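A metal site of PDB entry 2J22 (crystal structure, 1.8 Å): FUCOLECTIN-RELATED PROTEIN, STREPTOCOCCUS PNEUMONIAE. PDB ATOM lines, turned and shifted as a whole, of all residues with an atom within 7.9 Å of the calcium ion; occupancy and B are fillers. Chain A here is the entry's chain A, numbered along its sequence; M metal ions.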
ATOM      1  N   PHE A  31     -18.408  -4.574  -7.616  1.00  0.00           N
ATOM      2  CA  PHE A  31     -18.225  -3.267  -6.975  1.00  0.00           C
ATOM      3  C   PHE A  31     -17.202  -3.378  -5.855  1.00  0.00           C
ATOM      4  O   PHE A  31     -17.173  -4.364  -5.186  1.00  0.00           O
ATOM      5  CB  PHE A  31     -19.573  -2.682  -6.496  1.00  0.00           C
ATOM      6  CG  PHE A  31     -20.676  -2.828  -7.495  1.00  0.00           C
ATOM      7  CD1 PHE A  31     -20.528  -2.290  -8.770  1.00  0.00           C
ATOM      8  CD2 PHE A  31     -21.824  -3.566  -7.203  1.00  0.00           C
ATOM      9  CE1 PHE A  31     -21.515  -2.434  -9.740  1.00  0.00           C
ATOM     10  CE2 PHE A  31     -22.859  -3.716  -8.185  1.00  0.00           C
ATOM     11  CZ  PHE A  31     -22.682  -3.151  -9.454  1.00  0.00           C
ATOM     12  N   SER A  32     -16.392  -2.325  -5.682  1.00  0.00           N
ATOM     13  CA  SER A  32     -15.457  -2.204  -4.569  1.00  0.00           C
ATOM     14  C   SER A  32     -16.040  -2.539  -3.170  1.00  0.00           C
ATOM     15  O   SER A  32     -15.351  -3.165  -2.377  1.00  0.00           O
ATOM     16  CB  SER A  32     -14.652  -0.869  -4.610  1.00  0.00           C
ATOM     17  OG  SER A  32     -15.396   0.234  -4.099  1.00  0.00           O
ATOM     18  N   ARG A  33     -17.300  -2.223  -2.900  1.00  0.00           N
ATOM     19  CA  ARG A  33     -17.941  -2.413  -1.590  1.00  0.00           C
ATOM     20  C   ARG A  33     -18.084  -3.896  -1.249  1.00  0.00           C
ATOM     21  O   ARG A  33     -18.300  -4.240  -0.099  1.00  0.00           O
ATOM     22  CB  ARG A  33     -19.342  -1.759  -1.590  1.00  0.00           C
ATOM     23  CG  ARG A  33     -20.374  -2.356  -2.653  1.00  0.00           C
ATOM     24  CD  ARG A  33     -21.806  -1.931  -2.428  1.00  0.00           C
ATOM     25  NE  ARG A  33     -22.751  -2.511  -3.398  1.00  0.00           N
ATOM     26  CZ  ARG A  33     -23.143  -1.905  -4.509  1.00  0.00           C
ATOM     27  NH1 ARG A  33     -22.672  -0.702  -4.793  1.00  0.00           N
ATOM     28  NH2 ARG A  33     -24.011  -2.472  -5.316  1.00  0.00           N
ATOM     29  N   LEU A  34     -17.960  -4.764  -2.300  1.00  0.00           N
ATOM     30  CA  LEU A  34     -18.227  -6.192  -2.124  1.00  0.00           C
ATOM     31  C   LEU A  34     -17.119  -6.721  -1.263  1.00  0.00           C
ATOM     32  O   LEU A  34     -17.291  -7.803  -0.660  1.00  0.00           O
ATOM     33  CB  LEU A  34     -18.260  -6.940  -3.453  1.00  0.00           C
ATOM     34  CG  LEU A  34     -19.453  -6.506  -4.344  1.00  0.00           C
ATOM     35  CD1 LEU A  34     -19.583  -7.291  -5.645  1.00  0.00           C
ATOM     36  CD2 LEU A  34     -20.751  -6.571  -3.446  1.00  0.00           C
ATOM     37  N   ALA A  35     -15.988  -6.020  -1.197  1.00  0.00           N
ATOM     38  CA  ALA A  35     -14.925  -6.553  -0.305  1.00  0.00           C
ATOM     39  C   ALA A  35     -15.139  -6.158   1.178  1.00  0.00           C
ATOM     40  O   ALA A  35     -14.367  -6.533   2.046  1.00  0.00           O
ATOM     41  CB  ALA A  35     -13.467  -6.167  -0.780  1.00  0.00           C
ATOM     42  N   VAL A  36     -16.188  -5.393   1.489  1.00  0.00           N
ATOM     43  CA  VAL A  36     -16.427  -5.025   2.894  1.00  0.00           C
ATOM     44  C   VAL A  36     -17.909  -5.219   3.297  1.00  0.00           C
ATOM     45  O   VAL A  36     -18.408  -4.607   4.241  1.00  0.00           O
ATOM     46  CB  VAL A  36     -15.939  -3.583   3.216  1.00  0.00           C
ATOM     47  CG1 VAL A  36     -14.448  -3.410   2.918  1.00  0.00           C
ATOM     48  CG2 VAL A  36     -16.760  -2.496   2.410  1.00  0.00           C
ATOM     49  N   ASP A  37     -18.585  -6.115   2.617  1.00  0.00           N
ATOM     50  CA  ASP A  37     -19.980  -6.436   2.910  1.00  0.00           C
ATOM     51  C   ASP A  37     -20.225  -7.452   3.997  1.00  0.00           C
ATOM     52  O   ASP A  37     -21.416  -7.785   4.289  1.00  0.00           O
ATOM     53  CB  ASP A  37     -20.723  -6.832   1.635  1.00  0.00           C
ATOM     54  CG  ASP A  37     -20.284  -8.152   1.043  1.00  0.00           C
ATOM     55  OD1 ASP A  37     -19.324  -8.755   1.511  1.00  0.00           O
ATOM     56  OD2 ASP A  37     -20.838  -8.655   0.044  1.00  0.00           O
ATOM     57  N   GLY A  38     -19.130  -7.934   4.597  1.00  0.00           N
ATOM     58  CA  GLY A  38     -19.154  -8.963   5.616  1.00  0.00           C
ATOM     59  C   GLY A  38     -19.352 -10.395   5.128  1.00  0.00           C
ATOM     60  O   GLY A  38     -19.710 -11.244   5.916  1.00  0.00           O
ATOM     61  N   ASN A  39     -19.180 -10.673   3.838  1.00  0.00           N
ATOM     62  CA  ASN A  39     -19.432 -12.003   3.294  1.00  0.00           C
ATOM     63  C   ASN A  39     -18.147 -12.437   2.662  1.00  0.00           C
ATOM     64  O   ASN A  39     -17.674 -11.822   1.713  1.00  0.00           O
ATOM     65  CB  ASN A  39     -20.610 -11.974   2.282  1.00  0.00           C
ATOM     66  CG  ASN A  39     -20.931 -13.365   1.619  1.00  0.00           C
ATOM     67  OD1 ASN A  39     -20.256 -14.357   1.830  1.00  0.00           O
ATOM     68  ND2 ASN A  39     -21.973 -13.377   0.787  1.00  0.00           N
ATOM     69  N   LYS A  40     -17.539 -13.472   3.218  1.00  0.00           N
ATOM     70  CA  LYS A  40     -16.286 -13.960   2.704  1.00  0.00           C
ATOM     71  C   LYS A  40     -16.376 -14.979   1.573  1.00  0.00           C
ATOM     72  O   LYS A  40     -15.326 -15.504   1.133  1.00  0.00           O
ATOM     73  CB  LYS A  40     -15.504 -14.623   3.849  1.00  0.00           C
ATOM     74  CG  LYS A  40     -14.945 -13.597   4.827  1.00  0.00           C
ATOM     75  CD  LYS A  40     -14.492 -14.311   6.109  1.00  0.00           C
ATOM     76  CE  LYS A  40     -15.597 -14.407   7.138  1.00  0.00           C
ATOM     77  NZ  LYS A  40     -15.198 -15.346   8.237  1.00  0.00           N
ATOM     78  N   ASN A  41     -17.591 -15.297   1.107  1.00  0.00           N
ATOM     79  CA  ASN A  41     -17.740 -16.270  -0.008  1.00  0.00           C
ATOM     80  C   ASN A  41     -16.946 -15.783  -1.256  1.00  0.00           C
ATOM     81  O   ASN A  41     -17.146 -14.644  -1.787  1.00  0.00           O
ATOM     82  CB  ASN A  41     -19.266 -16.448  -0.337  1.00  0.00           C
ATOM     83  CG  ASN A  41     -19.526 -17.654  -1.237  1.00  0.00           C
ATOM     84  OD1 ASN A  41     -18.681 -18.015  -2.051  1.00  0.00           O
ATOM     85  ND2 ASN A  41     -20.672 -18.294  -1.050  1.00  0.00           N
ATOM     86  N   GLY A  42     -16.006 -16.600  -1.726  1.00  0.00           N
ATOM     87  CA  GLY A  42     -15.227 -16.217  -2.904  1.00  0.00           C
ATOM     88  C   GLY A  42     -15.738 -16.747  -4.232  1.00  0.00           C
ATOM     89  O   GLY A  42     -15.078 -16.604  -5.248  1.00  0.00           O
ATOM     90  N   HIS A  46     -21.914 -15.769  -6.207  1.00  0.00           N
ATOM     91  CA  HIS A  46     -22.527 -15.409  -4.945  1.00  0.00           C
ATOM     92  C   HIS A  46     -22.501 -13.899  -4.687  1.00  0.00           C
ATOM     93  O   HIS A  46     -22.961 -13.430  -3.637  1.00  0.00           O
ATOM     94  CB  HIS A  46     -22.006 -16.242  -3.787  1.00  0.00           C
ATOM     95  CG  HIS A  46     -22.686 -17.590  -3.694  1.00  0.00           C
ATOM     96  ND1 HIS A  46     -22.370 -18.644  -4.528  1.00  0.00           N
ATOM     97  CD2 HIS A  46     -23.704 -18.020  -2.915  1.00  0.00           C
ATOM     98  CE1 HIS A  46     -23.133 -19.681  -4.237  1.00  0.00           C
ATOM     99  NE2 HIS A  46     -23.959 -19.319  -3.265  1.00  0.00           N
ATOM    100  N   HIS A  47     -21.932 -13.163  -5.646  1.00  0.00           N
ATOM    101  CA  HIS A  47     -22.041 -11.712  -5.709  1.00  0.00           C
ATOM    102  C   HIS A  47     -21.372 -11.002  -4.542  1.00  0.00           C
ATOM    103  O   HIS A  47     -21.756  -9.899  -4.158  1.00  0.00           O
ATOM    104  CB  HIS A  47     -23.525 -11.297  -5.960  1.00  0.00           C
ATOM    105  CG  HIS A  47     -24.080 -11.732  -7.291  1.00  0.00           C
ATOM    106  ND1 HIS A  47     -25.411 -11.970  -7.509  1.00  0.00           N
ATOM    107  CD2 HIS A  47     -23.451 -11.993  -8.479  1.00  0.00           C
ATOM    108  CE1 HIS A  47     -25.598 -12.376  -8.761  1.00  0.00           C
ATOM    109  NE2 HIS A  47     -24.427 -12.393  -9.369  1.00  0.00           N
ATOM    110  N   SER A  48     -20.292 -11.597  -4.025  1.00  0.00           N
ATOM    111  CA  SER A  48     -19.567 -10.926  -2.946  1.00  0.00           C
ATOM    112  C   SER A  48     -18.073 -10.745  -3.222  1.00  0.00           C
ATOM    113  O   SER A  48     -17.284 -10.554  -2.301  1.00  0.00           O
ATOM    114  CB  SER A  48     -19.859 -11.611  -1.590  1.00  0.00           C
ATOM    115  OG  SER A  48     -19.700 -10.681  -0.523  1.00  0.00           O
ATOM    116  N   VAL A  49     -17.718 -10.715  -4.505  1.00  0.00           N
ATOM    117  CA  VAL A  49     -16.379 -10.534  -4.953  1.00  0.00           C
ATOM    118  C   VAL A  49     -16.236  -9.334  -5.916  1.00  0.00           C
ATOM    119  O   VAL A  49     -17.052  -9.184  -6.892  1.00  0.00           O
ATOM    120  CB  VAL A  49     -15.835 -11.889  -5.569  1.00  0.00           C
ATOM    121  CG1 VAL A  49     -14.335 -11.823  -5.954  1.00  0.00           C
ATOM    122  CG2 VAL A  49     -16.089 -12.991  -4.637  1.00  0.00           C
ATOM    123  N   THR A  50     -15.234  -8.475  -5.618  1.00  0.00           N
ATOM    124  CA  THR A  50     -14.938  -7.296  -6.439  1.00  0.00           C
ATOM    125  C   THR A  50     -14.304  -7.792  -7.786  1.00  0.00           C
ATOM    126  O   THR A  50     -13.852  -8.953  -7.924  1.00  0.00           O
ATOM    127  CB  THR A  50     -13.917  -6.320  -5.718  1.00  0.00           C
ATOM    128  OG1 THR A  50     -12.622  -6.897  -5.746  1.00  0.00           O
ATOM    129  CG2 THR A  50     -14.253  -6.065  -4.158  1.00  0.00           C
ATOM    130  N   TYR A  76      -9.254 -12.114   1.668  1.00  0.00           N
ATOM    131  CA  TYR A  76      -9.903 -13.342   1.188  1.00  0.00           C
ATOM    132  C   TYR A  76      -9.948 -13.270  -0.329  1.00  0.00           C
ATOM    133  O   TYR A  76     -10.353 -12.261  -0.886  1.00  0.00           O
ATOM    134  CB  TYR A  76     -11.313 -13.461   1.761  1.00  0.00           C
ATOM    135  CG  TYR A  76     -11.294 -13.907   3.208  1.00  0.00           C
ATOM    136  CD1 TYR A  76     -11.100 -15.240   3.515  1.00  0.00           C
ATOM    137  CD2 TYR A  76     -11.365 -12.979   4.260  1.00  0.00           C
ATOM    138  CE1 TYR A  76     -11.015 -15.678   4.814  1.00  0.00           C
ATOM    139  CE2 TYR A  76     -11.269 -13.424   5.603  1.00  0.00           C
ATOM    140  CZ  TYR A  76     -11.096 -14.777   5.843  1.00  0.00           C
ATOM    141  OH  TYR A  76     -11.052 -15.269   7.122  1.00  0.00           O
ATOM    142  N   LEU A 139     -11.276  -9.341  -5.150  1.00  0.00           N
ATOM    143  CA  LEU A 139     -11.216  -9.620  -3.717  1.00  0.00           C
ATOM    144  C   LEU A 139     -12.580 -10.075  -3.196  1.00  0.00           C
ATOM    145  O   LEU A 139     -13.568  -9.375  -3.322  1.00  0.00           O
ATOM    146  CB  LEU A 139     -10.731  -8.330  -3.001  1.00  0.00           C
ATOM    147  CG  LEU A 139      -9.449  -7.615  -3.486  1.00  0.00           C
ATOM    148  CD1 LEU A 139      -9.153  -6.253  -2.962  1.00  0.00           C
ATOM    149  CD2 LEU A 139      -8.344  -8.423  -2.824  1.00  0.00           C
ATOM    150  N   ALA A 140     -12.656 -11.204  -2.518  1.00  0.00           N
ATOM    151  CA  ALA A 140     -13.893 -11.601  -1.823  1.00  0.00           C
ATOM    152  C   ALA A 140     -14.160 -10.779  -0.560  1.00  0.00           C
ATOM    153  O   ALA A 140     -15.328 -10.454  -0.247  1.00  0.00           O
ATOM    154  CB  ALA A 140     -13.834 -13.109  -1.422  1.00  0.00           C
ATOM    155  N   GLU A 141     -13.101 -10.485   0.209  1.00  0.00           N
ATOM    156  CA  GLU A 141     -13.199  -9.730   1.423  1.00  0.00           C
ATOM    157  C   GLU A 141     -11.821  -9.216   1.893  1.00  0.00           C
ATOM    158  O   GLU A 141     -10.756  -9.901   1.801  1.00  0.00           O
ATOM    159  CB  GLU A 141     -13.967 -10.539   2.521  1.00  0.00           C
ATOM    160  CG  GLU A 141     -14.409  -9.722   3.721  1.00  0.00           C
ATOM    161  CD  GLU A 141     -15.732  -8.990   3.481  1.00  0.00           C
ATOM    162  OE1 GLU A 141     -16.254  -9.049   2.365  1.00  0.00           O
ATOM    163  OE2 GLU A 141     -16.219  -8.378   4.438  1.00  0.00           O
ATOM    164  N   VAL A 142     -11.835  -8.006   2.396  1.00  0.00           N
ATOM    165  CA  VAL A 142     -10.653  -7.415   3.053  1.00  0.00           C
ATOM    166  C   VAL A 142     -11.143  -7.012   4.447  1.00  0.00           C
ATOM    167  O   VAL A 142     -12.020  -6.209   4.573  1.00  0.00           O
ATOM    168  CB  VAL A 142     -10.092  -6.145   2.274  1.00  0.00           C
ATOM    169  CG1 VAL A 142      -8.951  -5.430   3.042  1.00  0.00           C
ATOM    170  CG2 VAL A 142      -9.670  -6.475   0.820  1.00  0.00           C
HETATM  171 CA    CA M   1     -17.421  -9.982   0.267  1.00  0.00          CA
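Of the 22 residues printed, 6 come within 4 Å of the calcium ion.
The nearest printed residue that does not touch the calcium ion is Ala 35 (4.3 Å).
The backbone NH (N) of Tyr 76 is in hydrogen-bond range of the backbone carbonyl oxygen (O) of Glu 141, at 2.7 Å.
OD1 of Asn 39 lies within hydrogen-bond range of N of Asn 41.
The side-chain carboxylate (OE2) of Glu 141 is in hydrogen-bond range of the backbone NH (N) of Gly 38, 2.9 Å away.
The backbone NH of Ala 140 lies within hydrogen-bond range of the backbone carbonyl oxygen of Tyr 76 (3.0 Å).
The calcium ion is bound by the backbone carbonyl oxygen of Ala 140 (2.2 Å), the backbone carbonyl oxygen of Asn 39 (2.4 Å), the backbone carbonyl oxygen of Leu 34 (2.4 Å), the side-chain hydroxyl of Ser 48 (2.5 Å), the side-chain carboxylate of Glu 141 (2.6 Å), the side-chain carboxylate of Asp 37 (2.6 Å) and the backbone carbonyl oxygen of Ser 48 (2.6 Å).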
